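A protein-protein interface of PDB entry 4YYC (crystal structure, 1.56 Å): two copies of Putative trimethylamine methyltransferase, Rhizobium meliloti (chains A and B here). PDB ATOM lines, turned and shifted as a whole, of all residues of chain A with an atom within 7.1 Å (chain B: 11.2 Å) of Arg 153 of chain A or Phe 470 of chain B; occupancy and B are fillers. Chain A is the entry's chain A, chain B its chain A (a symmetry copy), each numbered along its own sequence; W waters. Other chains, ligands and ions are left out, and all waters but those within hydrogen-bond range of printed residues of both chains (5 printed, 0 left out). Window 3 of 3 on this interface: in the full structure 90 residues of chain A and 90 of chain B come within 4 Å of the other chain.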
ATOM      1  N   PHE A 145       0.564  -1.533 -25.426  1.00  0.00           N
ATOM      2  CA  PHE A 145      -0.250  -0.845 -26.420  1.00  0.00           C
ATOM      3  C   PHE A 145      -0.937   0.354 -25.825  1.00  0.00           C
ATOM      4  O   PHE A 145      -1.218   0.407 -24.627  1.00  0.00           O
ATOM      5  CB  PHE A 145      -1.350  -1.770 -26.980  1.00  0.00           C
ATOM      6  CG  PHE A 145      -0.832  -2.967 -27.728  1.00  0.00           C
ATOM      7  CD1 PHE A 145      -0.418  -2.854 -29.052  1.00  0.00           C
ATOM      8  CD2 PHE A 145      -0.722  -4.182 -27.089  1.00  0.00           C
ATOM      9  CE1 PHE A 145       0.058  -3.988 -29.728  1.00  0.00           C
ATOM     10  CE2 PHE A 145      -0.240  -5.305 -27.754  1.00  0.00           C
ATOM     11  CZ  PHE A 145       0.151  -5.197 -29.065  1.00  0.00           C
ATOM     12  N   VAL A 146      -1.231   1.315 -26.694  1.00  0.00           N
ATOM     13  CA  VAL A 146      -2.164   2.390 -26.357  1.00  0.00           C
ATOM     14  C   VAL A 146      -3.374   2.345 -27.259  1.00  0.00           C
ATOM     15  O   VAL A 146      -3.307   1.802 -28.385  1.00  0.00           O
ATOM     16  CB  VAL A 146      -1.538   3.807 -26.420  1.00  0.00           C
ATOM     17  CG1 VAL A 146      -0.425   3.904 -25.389  1.00  0.00           C
ATOM     18  CG2 VAL A 146      -1.038   4.140 -27.823  1.00  0.00           C
ATOM     19  N   ARG A 147      -4.481   2.910 -26.769  1.00  0.00           N
ATOM     20  CA  ARG A 147      -5.540   3.361 -27.637  1.00  0.00           C
ATOM     21  C   ARG A 147      -5.433   4.850 -27.716  1.00  0.00           C
ATOM     22  O   ARG A 147      -5.666   5.521 -26.697  1.00  0.00           O
ATOM     23  CB  ARG A 147      -6.892   2.966 -27.070  1.00  0.00           C
ATOM     24  CG  ARG A 147      -7.309   1.642 -27.524  1.00  0.00           C
ATOM     25  CD  ARG A 147      -7.966   1.640 -28.902  1.00  0.00           C
ATOM     26  NE  ARG A 147      -8.520   0.346 -29.102  1.00  0.00           N
ATOM     27  CZ  ARG A 147      -9.054  -0.079 -30.218  1.00  0.00           C
ATOM     28  NH1 ARG A 147      -9.083   0.674 -31.316  1.00  0.00           N
ATOM     29  NH2 ARG A 147      -9.526  -1.298 -30.237  1.00  0.00           N
ATOM     30  N   ASP A 148      -4.984   5.347 -28.870  1.00  0.00           N
ATOM     31  CA  ASP A 148      -4.611   6.759 -28.964  1.00  0.00           C
ATOM     32  C   ASP A 148      -5.853   7.642 -29.144  1.00  0.00           C
ATOM     33  O   ASP A 148      -6.961   7.146 -29.236  1.00  0.00           O
ATOM     34  CB  ASP A 148      -3.499   7.004 -29.971  1.00  0.00           C
ATOM     35  CG  ASP A 148      -3.913   6.846 -31.422  1.00  0.00           C
ATOM     36  OD1 ASP A 148      -5.110   6.897 -31.735  1.00  0.00           O
ATOM     37  OD2 ASP A 148      -2.965   6.648 -32.254  1.00  0.00           O
ATOM     38  N   ASP A 150      -6.749   9.232 -31.635  1.00  0.00           N
ATOM     39  CA  ASP A 150      -7.369   9.058 -32.965  1.00  0.00           C
ATOM     40  C   ASP A 150      -8.058   7.708 -33.131  1.00  0.00           C
ATOM     41  O   ASP A 150      -8.484   7.371 -34.250  1.00  0.00           O
ATOM     42  CB  ASP A 150      -6.315   9.260 -34.054  1.00  0.00           C
ATOM     43  CG  ASP A 150      -5.800  10.669 -34.080  1.00  0.00           C
ATOM     44  OD1 ASP A 150      -6.607  11.607 -34.000  1.00  0.00           O
ATOM     45  OD2 ASP A 150      -4.591  10.852 -34.129  1.00  0.00           O
ATOM     46  N   GLY A 151      -8.133   6.940 -32.056  1.00  0.00           N
ATOM     47  CA  GLY A 151      -8.786   5.629 -32.029  1.00  0.00           C
ATOM     48  C   GLY A 151      -7.936   4.429 -32.464  1.00  0.00           C
ATOM     49  O   GLY A 151      -8.466   3.312 -32.618  1.00  0.00           O
ATOM     50  N   ASN A 152      -6.638   4.618 -32.637  1.00  0.00           N
ATOM     51  CA  ASN A 152      -5.809   3.537 -33.106  1.00  0.00           C
ATOM     52  C   ASN A 152      -5.294   2.729 -31.922  1.00  0.00           C
ATOM     53  O   ASN A 152      -4.834   3.306 -30.908  1.00  0.00           O
ATOM     54  CB  ASN A 152      -4.593   4.063 -33.836  1.00  0.00           C
ATOM     55  CG  ASN A 152      -4.935   4.956 -35.016  1.00  0.00           C
ATOM     56  OD1 ASN A 152      -4.541   6.140 -35.072  1.00  0.00           O
ATOM     57  ND2 ASN A 152      -5.658   4.417 -35.943  1.00  0.00           N
ATOM     58  N   ARG A 153      -5.372   1.410 -32.041  1.00  0.00           N
ATOM     59  CA  ARG A 153      -4.673   0.520 -31.115  1.00  0.00           C
ATOM     60  C   ARG A 153      -3.303   0.269 -31.717  1.00  0.00           C
ATOM     61  O   ARG A 153      -3.209  -0.321 -32.799  1.00  0.00           O
ATOM     62  CB  ARG A 153      -5.412  -0.791 -30.937  1.00  0.00           C
ATOM     63  CG  ARG A 153      -4.879  -1.728 -29.884  1.00  0.00           C
ATOM     64  CD  ARG A 153      -5.658  -3.017 -29.852  1.00  0.00           C
ATOM     65  NE  ARG A 153      -5.186  -4.012 -28.919  1.00  0.00           N
ATOM     66  CZ  ARG A 153      -4.221  -4.893 -29.147  1.00  0.00           C
ATOM     67  NH1 ARG A 153      -3.532  -4.876 -30.294  1.00  0.00           N
ATOM     68  NH2 ARG A 153      -3.950  -5.802 -28.244  1.00  0.00           N
ATOM     69  N   ARG A 154      -2.254   0.653 -31.012  1.00  0.00           N
ATOM     70  CA  ARG A 154      -0.900   0.568 -31.570  1.00  0.00           C
ATOM     71  C   ARG A 154       0.111   0.443 -30.456  1.00  0.00           C
ATOM     72  O   ARG A 154      -0.209   0.736 -29.295  1.00  0.00           O
ATOM     73  CB  ARG A 154      -0.644   1.788 -32.419  1.00  0.00           C
ATOM     74  CG  ARG A 154      -0.775   3.110 -31.683  1.00  0.00           C
ATOM     75  CD  ARG A 154      -0.190   4.270 -32.464  1.00  0.00           C
ATOM     76  NE  ARG A 154      -0.423   5.535 -31.772  1.00  0.00           N
ATOM     77  CZ  ARG A 154       0.265   5.958 -30.697  1.00  0.00           C
ATOM     78  NH1 ARG A 154       1.250   5.240 -30.160  1.00  0.00           N
ATOM     79  NH2 ARG A 154      -0.054   7.101 -30.139  1.00  0.00           N
ATOM     80  N   TYR A 155       1.365   0.084 -30.769  1.00  0.00           N
ATOM     81  CA  TYR A 155       2.381   0.062 -29.711  1.00  0.00           C
ATOM     82  C   TYR A 155       2.576   1.435 -29.128  1.00  0.00           C
ATOM     83  O   TYR A 155       2.532   2.457 -29.847  1.00  0.00           O
ATOM     84  CB  TYR A 155       3.749  -0.419 -30.260  1.00  0.00           C
ATOM     85  CG  TYR A 155       3.750  -1.888 -30.487  1.00  0.00           C
ATOM     86  CD1 TYR A 155       3.867  -2.732 -29.437  1.00  0.00           C
ATOM     87  CD2 TYR A 155       3.579  -2.434 -31.748  1.00  0.00           C
ATOM     88  CE1 TYR A 155       3.866  -4.098 -29.609  1.00  0.00           C
ATOM     89  CE2 TYR A 155       3.559  -3.809 -31.925  1.00  0.00           C
ATOM     90  CZ  TYR A 155       3.700  -4.618 -30.845  1.00  0.00           C
ATOM     91  OH  TYR A 155       3.705  -5.986 -30.910  1.00  0.00           O
ATOM     92  N   LYS A 364     -12.463  -4.417 -24.482  1.00  0.00           N
ATOM     93  CA  LYS A 364     -11.580  -3.848 -25.492  1.00  0.00           C
ATOM     94  C   LYS A 364     -11.820  -2.365 -25.745  1.00  0.00           C
ATOM     95  O   LYS A 364     -11.029  -1.711 -26.426  1.00  0.00           O
ATOM     96  CB  LYS A 364     -11.688  -4.645 -26.801  1.00  0.00           C
ATOM     97  CG  LYS A 364     -10.778  -5.877 -26.858  1.00  0.00           C
ATOM     98  CD  LYS A 364     -10.885  -6.890 -25.758  1.00  0.00           C
ATOM     99  CE  LYS A 364     -12.215  -7.573 -25.729  1.00  0.00           C
ATOM    100  NZ  LYS A 364     -12.281  -8.540 -24.604  1.00  0.00           N
ATOM    101  N   GLU A 397      -8.469  -3.644 -21.661  1.00  0.00           N
ATOM    102  CA  GLU A 397      -8.113  -4.834 -22.376  1.00  0.00           C
ATOM    103  C   GLU A 397      -7.230  -5.725 -21.511  1.00  0.00           C
ATOM    104  O   GLU A 397      -6.214  -6.255 -21.948  1.00  0.00           O
ATOM    105  CB  GLU A 397      -7.474  -4.488 -23.752  1.00  0.00           C
ATOM    106  CG  GLU A 397      -7.555  -5.628 -24.723  1.00  0.00           C
ATOM    107  CD  GLU A 397      -6.756  -5.367 -25.971  1.00  0.00           C
ATOM    108  OE1 GLU A 397      -7.065  -4.393 -26.720  1.00  0.00           O
ATOM    109  OE2 GLU A 397      -5.774  -6.090 -26.199  1.00  0.00           O
ATOM    110  N   LEU A 400      -3.403  -4.948 -21.348  1.00  0.00           N
ATOM    111  CA  LEU A 400      -2.613  -4.798 -22.565  1.00  0.00           C
ATOM    112  C   LEU A 400      -2.634  -3.419 -23.120  1.00  0.00           C
ATOM    113  O   LEU A 400      -1.778  -3.076 -23.946  1.00  0.00           O
ATOM    114  CB  LEU A 400      -3.081  -5.780 -23.653  1.00  0.00           C
ATOM    115  CG  LEU A 400      -2.708  -7.221 -23.471  1.00  0.00           C
ATOM    116  CD1 LEU A 400      -3.371  -8.086 -24.520  1.00  0.00           C
ATOM    117  CD2 LEU A 400      -1.197  -7.394 -23.538  1.00  0.00           C
ATOM    118  N   VAL A 401      -3.622  -2.610 -22.702  1.00  0.00           N
ATOM    119  CA  VAL A 401      -3.793  -1.270 -23.252  1.00  0.00           C
ATOM    120  C   VAL A 401      -3.853  -0.185 -22.191  1.00  0.00           C
ATOM    121  O   VAL A 401      -4.560  -0.344 -21.197  1.00  0.00           O
ATOM    122  CB  VAL A 401      -5.090  -1.234 -24.099  1.00  0.00           C
ATOM    123  CG1 VAL A 401      -5.487   0.172 -24.492  1.00  0.00           C
ATOM    124  CG2 VAL A 401      -4.902  -2.105 -25.343  1.00  0.00           C
ATOM    125  N   ASP B 466     -17.417  -9.517 -22.820  1.00  0.00           N
ATOM    126  CA  ASP B 466     -16.501 -10.080 -23.755  1.00  0.00           C
ATOM    127  C   ASP B 466     -15.120 -10.158 -23.099  1.00  0.00           C
ATOM    128  O   ASP B 466     -14.494  -9.138 -22.758  1.00  0.00           O
ATOM    129  CB  ASP B 466     -16.439  -9.264 -25.045  1.00  0.00           C
ATOM    130  CG  ASP B 466     -15.575  -9.901 -26.073  1.00  0.00           C
ATOM    131  OD1 ASP B 466     -14.366 -10.103 -25.801  1.00  0.00           O
ATOM    132  OD2 ASP B 466     -16.077 -10.257 -27.202  1.00  0.00           O
ATOM    133  N   ASN B 467     -14.662 -11.394 -22.910  1.00  0.00           N
ATOM    134  CA  ASN B 467     -13.409 -11.656 -22.267  1.00  0.00           C
ATOM    135  C   ASN B 467     -12.392 -12.263 -23.241  1.00  0.00           C
ATOM    136  O   ASN B 467     -11.387 -12.877 -22.838  1.00  0.00           O
ATOM    137  CB  ASN B 467     -13.661 -12.628 -21.107  1.00  0.00           C
ATOM    138  CG  ASN B 467     -14.547 -12.026 -20.046  1.00  0.00           C
ATOM    139  OD1 ASN B 467     -15.571 -12.618 -19.665  1.00  0.00           O
ATOM    140  ND2 ASN B 467     -14.200 -10.857 -19.603  1.00  0.00           N
ATOM    141  N   ASN B 468     -12.640 -12.094 -24.528  1.00  0.00           N
ATOM    142  CA  ASN B 468     -11.768 -12.647 -25.547  1.00  0.00           C
ATOM    143  C   ASN B 468     -10.607 -11.732 -25.903  1.00  0.00           C
ATOM    144  O   ASN B 468     -10.579 -10.557 -25.530  1.00  0.00           O
ATOM    145  CB  ASN B 468     -12.597 -12.973 -26.778  1.00  0.00           C
ATOM    146  CG  ASN B 468     -13.566 -14.107 -26.522  1.00  0.00           C
ATOM    147  OD1 ASN B 468     -13.294 -15.010 -25.705  1.00  0.00           O
ATOM    148  ND2 ASN B 468     -14.689 -14.077 -27.194  1.00  0.00           N
ATOM    149  N   SER B 469      -9.640 -12.264 -26.632  1.00  0.00           N
ATOM    150  CA  SER B 469      -8.548 -11.416 -27.139  1.00  0.00           C
ATOM    151  C   SER B 469      -9.059 -10.312 -28.017  1.00  0.00           C
ATOM    152  O   SER B 469     -10.135 -10.430 -28.605  1.00  0.00           O
ATOM    153  CB  SER B 469      -7.570 -12.252 -27.985  1.00  0.00           C
ATOM    154  OG  SER B 469      -8.206 -12.754 -29.169  1.00  0.00           O
ATOM    155  N   PHE B 470      -8.284  -9.245 -28.151  1.00  0.00           N
ATOM    156  CA  PHE B 470      -8.558  -8.192 -29.143  1.00  0.00           C
ATOM    157  C   PHE B 470      -8.825  -8.789 -30.519  1.00  0.00           C
ATOM    158  O   PHE B 470      -9.772  -8.429 -31.206  1.00  0.00           O
ATOM    159  CB  PHE B 470      -7.398  -7.164 -29.227  1.00  0.00           C
ATOM    160  CG  PHE B 470      -7.498  -6.265 -30.396  1.00  0.00           C
ATOM    161  CD1 PHE B 470      -8.441  -5.271 -30.449  1.00  0.00           C
ATOM    162  CD2 PHE B 470      -6.684  -6.459 -31.485  1.00  0.00           C
ATOM    163  CE1 PHE B 470      -8.556  -4.456 -31.559  1.00  0.00           C
ATOM    164  CE2 PHE B 470      -6.784  -5.650 -32.591  1.00  0.00           C
ATOM    165  CZ  PHE B 470      -7.726  -4.662 -32.630  1.00  0.00           C
ATOM    166  N   GLU B 471      -7.984  -9.734 -30.929  1.00  0.00           N
ATOM    167  CA  GLU B 471      -8.078 -10.303 -32.263  1.00  0.00           C
ATOM    168  C   GLU B 471      -9.405 -11.002 -32.469  1.00  0.00           C
ATOM    169  O   GLU B 471     -10.022 -10.828 -33.504  1.00  0.00           O
ATOM    170  CB  GLU B 471      -6.911 -11.233 -32.551  1.00  0.00           C
ATOM    171  CG  GLU B 471      -5.568 -10.532 -32.727  1.00  0.00           C
ATOM    172  CD  GLU B 471      -4.924 -10.014 -31.451  1.00  0.00           C
ATOM    173  OE1 GLU B 471      -5.247 -10.487 -30.311  1.00  0.00           O
ATOM    174  OE2 GLU B 471      -4.057  -9.107 -31.688  1.00  0.00           O
ATOM    175  N   GLN B 472      -9.857 -11.791 -31.517  1.00  0.00           N
ATOM    176  CA  GLN B 472     -11.132 -12.438 -31.648  1.00  0.00           C
ATOM    177  C   GLN B 472     -12.290 -11.449 -31.645  1.00  0.00           C
ATOM    178  O   GLN B 472     -13.205 -11.522 -32.432  1.00  0.00           O
ATOM    179  CB  GLN B 472     -11.327 -13.499 -30.570  1.00  0.00           C
ATOM    180  CG  GLN B 472     -12.681 -14.197 -30.708  1.00  0.00           C
ATOM    181  CD  GLN B 472     -12.886 -15.391 -29.797  1.00  0.00           C
ATOM    182  OE1 GLN B 472     -12.000 -15.783 -29.047  1.00  0.00           O
ATOM    183  NE2 GLN B 472     -14.074 -15.975 -29.867  1.00  0.00           N
ATOM    184  N   TRP B 473     -12.212 -10.467 -30.760  1.00  0.00           N
ATOM    185  CA  TRP B 473     -13.270  -9.464 -30.644  1.00  0.00           C
ATOM    186  C   TRP B 473     -13.381  -8.618 -31.928  1.00  0.00           C
ATOM    187  O   TRP B 473     -14.482  -8.283 -32.368  1.00  0.00           O
ATOM    188  CB  TRP B 473     -13.004  -8.613 -29.400  1.00  0.00           C
ATOM    189  CG  TRP B 473     -13.832  -7.362 -29.236  1.00  0.00           C
ATOM    190  CD1 TRP B 473     -15.034  -7.240 -28.605  1.00  0.00           C
ATOM    191  CD2 TRP B 473     -13.471  -6.049 -29.683  1.00  0.00           C
ATOM    192  NE1 TRP B 473     -15.425  -5.898 -28.607  1.00  0.00           N
ATOM    193  CE2 TRP B 473     -14.487  -5.166 -29.277  1.00  0.00           C
ATOM    194  CE3 TRP B 473     -12.367  -5.535 -30.339  1.00  0.00           C
ATOM    195  CZ2 TRP B 473     -14.455  -3.795 -29.581  1.00  0.00           C
ATOM    196  CZ3 TRP B 473     -12.328  -4.168 -30.620  1.00  0.00           C
ATOM    197  CH2 TRP B 473     -13.362  -3.320 -30.232  1.00  0.00           C
ATOM    198  N   GLU B 474     -12.253  -8.349 -32.569  1.00  0.00           N
ATOM    199  CA  GLU B 474     -12.228  -7.608 -33.851  1.00  0.00           C
ATOM    200  C   GLU B 474     -12.855  -8.474 -34.942  1.00  0.00           C
ATOM    201  O   GLU B 474     -13.676  -7.970 -35.729  1.00  0.00           O
ATOM    202  CB  GLU B 474     -10.789  -7.193 -34.190  1.00  0.00           C
ATOM    203  CG  GLU B 474     -10.661  -6.386 -35.465  1.00  0.00           C
ATOM    204  CD  GLU B 474      -9.211  -6.106 -35.866  1.00  0.00           C
ATOM    205  OE1 GLU B 474      -8.297  -6.937 -35.689  1.00  0.00           O
ATOM    206  OE2 GLU B 474      -8.997  -5.018 -36.429  1.00  0.00           O
ATOM    207  N   ILE B 475     -12.514  -9.773 -34.992  1.00  0.00           N
ATOM    208  CA  ILE B 475     -13.154 -10.736 -35.931  1.00  0.00           C
ATOM    209  C   ILE B 475     -14.681 -10.794 -35.765  1.00  0.00           C
ATOM    210  O   ILE B 475     -15.439 -10.874 -36.744  1.00  0.00           O
ATOM    211  CB  ILE B 475     -12.540 -12.147 -35.743  1.00  0.00           C
ATOM    212  CG1 ILE B 475     -11.135 -12.158 -36.321  1.00  0.00           C
ATOM    213  CG2 ILE B 475     -13.371 -13.270 -36.356  1.00  0.00           C
ATOM    214  CD1 ILE B 475     -10.294 -13.324 -35.856  1.00  0.00           C
ATOM    215  N   GLU B 476     -15.107 -10.683 -34.518  1.00  0.00           N
ATOM    216  CA  GLU B 476     -16.518 -10.722 -34.184  1.00  0.00           C
ATOM    217  C   GLU B 476     -17.186  -9.348 -34.231  1.00  0.00           C
ATOM    218  O   GLU B 476     -18.228  -9.179 -33.588  1.00  0.00           O
ATOM    219  CB  GLU B 476     -16.706 -11.389 -32.848  1.00  0.00           C
ATOM    220  CG  GLU B 476     -16.220 -12.825 -32.877  1.00  0.00           C
ATOM    221  CD  GLU B 476     -16.426 -13.656 -31.634  1.00  0.00           C
ATOM    222  OE1 GLU B 476     -16.878 -13.161 -30.596  1.00  0.00           O
ATOM    223  OE2 GLU B 476     -16.093 -14.852 -31.723  1.00  0.00           O
ATOM    224  N   GLY B 477     -16.612  -8.350 -34.897  1.00  0.00           N
ATOM    225  CA  GLY B 477     -17.314  -7.105 -35.219  1.00  0.00           C
ATOM    226  C   GLY B 477     -17.080  -5.939 -34.277  1.00  0.00           C
ATOM    227  O   GLY B 477     -17.808  -4.939 -34.373  1.00  0.00           O
ATOM    228  N   GLU B 478     -16.055  -6.018 -33.444  1.00  0.00           N
ATOM    229  CA  GLU B 478     -15.727  -4.893 -32.583  1.00  0.00           C
ATOM    230  C   GLU B 478     -16.970  -4.401 -31.812  1.00  0.00           C
ATOM    231  O   GLU B 478     -17.236  -3.210 -31.729  1.00  0.00           O
ATOM    232  CB  GLU B 478     -15.100  -3.758 -33.363  1.00  0.00           C
ATOM    233  CG  GLU B 478     -13.791  -4.172 -34.055  1.00  0.00           C
ATOM    234  CD  GLU B 478     -13.191  -3.065 -34.894  1.00  0.00           C
ATOM    235  OE1 GLU B 478     -12.770  -2.039 -34.339  1.00  0.00           O
ATOM    236  OE2 GLU B 478     -13.113  -3.235 -36.089  1.00  0.00           O
ATOM    237  N   LYS B 479     -17.680  -5.345 -31.220  1.00  0.00           N
ATOM    238  CA  LYS B 479     -18.978  -5.039 -30.599  1.00  0.00           C
ATOM    239  C   LYS B 479     -18.873  -4.480 -29.190  1.00  0.00           C
ATOM    240  O   LYS B 479     -18.132  -5.005 -28.348  1.00  0.00           O
ATOM    241  CB  LYS B 479     -19.846  -6.288 -30.571  1.00  0.00           C
ATOM    242  CG  LYS B 479     -20.260  -6.829 -31.922  1.00  0.00           C
ATOM    243  CD  LYS B 479     -21.059  -8.080 -31.814  1.00  0.00           C
ATOM    244  CE  LYS B 479     -21.499  -8.519 -33.212  1.00  0.00           C
ATOM    245  NZ  LYS B 479     -22.328  -9.731 -33.183  1.00  0.00           N
ATOM    246  N   ARG B 484     -24.307  -6.775 -27.891  1.00  0.00           N
ATOM    247  CA  ARG B 484     -24.534  -8.132 -27.424  1.00  0.00           C
ATOM    248  C   ARG B 484     -25.825  -8.221 -26.555  1.00  0.00           C
ATOM    249  O   ARG B 484     -26.542  -9.229 -26.599  1.00  0.00           O
ATOM    250  CB  ARG B 484     -23.295  -8.704 -26.722  1.00  0.00           C
ATOM    251  CG  ARG B 484     -22.046  -8.808 -27.603  1.00  0.00           C
ATOM    252  CD  ARG B 484     -20.921  -9.594 -26.922  1.00  0.00           C
ATOM    253  NE  ARG B 484     -20.419  -8.868 -25.753  1.00  0.00           N
ATOM    254  CZ  ARG B 484     -19.675  -7.775 -25.740  1.00  0.00           C
ATOM    255  NH1 ARG B 484     -19.178  -7.244 -26.855  1.00  0.00           N
ATOM    256  NH2 ARG B 484     -19.415  -7.214 -24.588  1.00  0.00           N
HETATM  257  O   HOH W   1     -10.668  -1.680 -32.591  1.00  0.00           O
HETATM  258  O   HOH W   2     -14.940  -5.447 -25.615  1.00  0.00           O
HETATM  259  O   HOH W   3      -2.140  -7.475 -30.685  1.00  0.00           O
HETATM  260  O   HOH W   4     -10.737  -9.957 -22.515  1.00  0.00           O
HETATM  261  O   HOH W   5      -6.202  -8.806 -26.278  1.00  0.00           O
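OD1 of Asp 466 of chain B is in salt-bridge range of NZ of Lys 364 of chain A.
The backbone carbonyl oxygen of Asn 468 of chain B is in hydrogen-bond range of the side-chain amino group of Lys 364 of chain A.
The guanidinium group (NH1) of Arg 147 of chain A is in hydrogen-bond range of the backbone carbonyl oxygen (O) of Gly 151 of chain A, at 3.0 Å.
The guanidinium group (NH2) of Arg 153 of chain A is in salt-bridge range of the side-chain carboxylate (OE2) of Glu 397 of chain A.
OD1 of Asp 466 of chain B is in hydrogen-bond range of N of Asn 468 of chain B (2.9 Å).
ND2 of Asn 468 of chain B sits close to NE2 of Gln 472 of chain B (3.3 Å).
O of Trp 473 of chain B is in hydrogen-bond range of N of Glu 478 of chain B (3.0 Å).
The indole nitrogen (NE1) of Trp 473 of chain B is in hydrogen-bond range of the backbone carbonyl oxygen (O) of Lys 479 of chain B (2.9 Å).
Arg 147 of chain A touches Phe 470 of chain B (NH2 to CE1, 3.6 Å).
Arg 153 of chain A touches Phe 470 of chain B.
Asn 467 of chain B touches Lys 364 of chain A.
CG of Lys 364 of chain A touches CA of Phe 470 of chain B (3.9 Å).
Trp 473 of chain B touches Lys 364 of chain A.
Glu 397 of chain A touches Phe 470 of chain B (OE2 to CB, 3.6 Å).
No residue of chain B comes within 4 Å of Phe 145 of chain A.
No residue of chain B comes within 4 Å of Gly 151 of chain A.
Of chain B, only Phe 470 comes within 4 Å of Arg 153 of chain A.
Of the printed residues of chain B, Glu 397 of chain A touches Phe 470.
No residue of chain B comes within 4 Å of Leu 400 of chain A.
Of the printed residues of chain A, Asp 466 of chain B touches Lys 364 (2.9 Å).
Of the printed residues of chain A, Asn 468 of chain B touches Lys 364.
Of the printed residues of chain A, Trp 473 of chain B touches Lys 364.
Ile 475 of chain B touches none of the printed residues of chain A.
The nearest residue of chain B that does not touch Arg 153 of chain A is Glu 471 of chain B (4.5 Å).
The nearest residue of chain A that does not touch Phe 470 of chain B is Leu 400 of chain A (6.2 Å).
The nearest printed residue of chain A that does not touch Asn 467 of chain B is Glu 397 of chain A (8.3 Å).
Hydrophobic or aromatic side chains of chain B that line the printed part of chain A: Phe 470 and Trp 473.
Of the 14 printed residues of chain A, 4 touch a printed residue of chain B.
Among the printed residues, 8 pairs touch across the chains.
Among the printed residues, Asp or Glu carboxylates within 4 Å of a Lys or Arg side-chain nitrogen of the other chain: Lys 364 of chain A with Asp 466 of chain B.
No position is printed for both chains.
Of the 8 pairs that touch across the chains among the printed residues, none has its exchanged pair printed and touching as well.
Water W1 bridges NH2 of Arg 147 of chain A (2.6 Å) and OE1 of Glu 478 of chain B (2.8 Å).
Water W3 lies within hydrogen-bond range of the side-chain carboxylate (OE2) of Glu 471 of chain B (2.7 Å) and the guanidinium group (NH1) of Arg 153 of chain A (3.0 Å).
Water W5 lies within hydrogen-bond range of the side-chain carboxylate (OE2) of Glu 397 of chain A (2.8 Å) and the backbone NH (N) of Phe 470 of chain B (2.8 Å).
Water W2 bridges the backbone NH (N) of Lys 364 of chain A and the indole nitrogen (NE1) of Trp 473 of chain B.
Water W4 lies within hydrogen-bond range of the side-chain amino group of Lys 364 of chain A (3.0 Å), the backbone carbonyl oxygen of Asn 467 of chain B (3.0 Å) and the backbone carbonyl oxygen of Asn 468 of chain B (3.1 Å).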
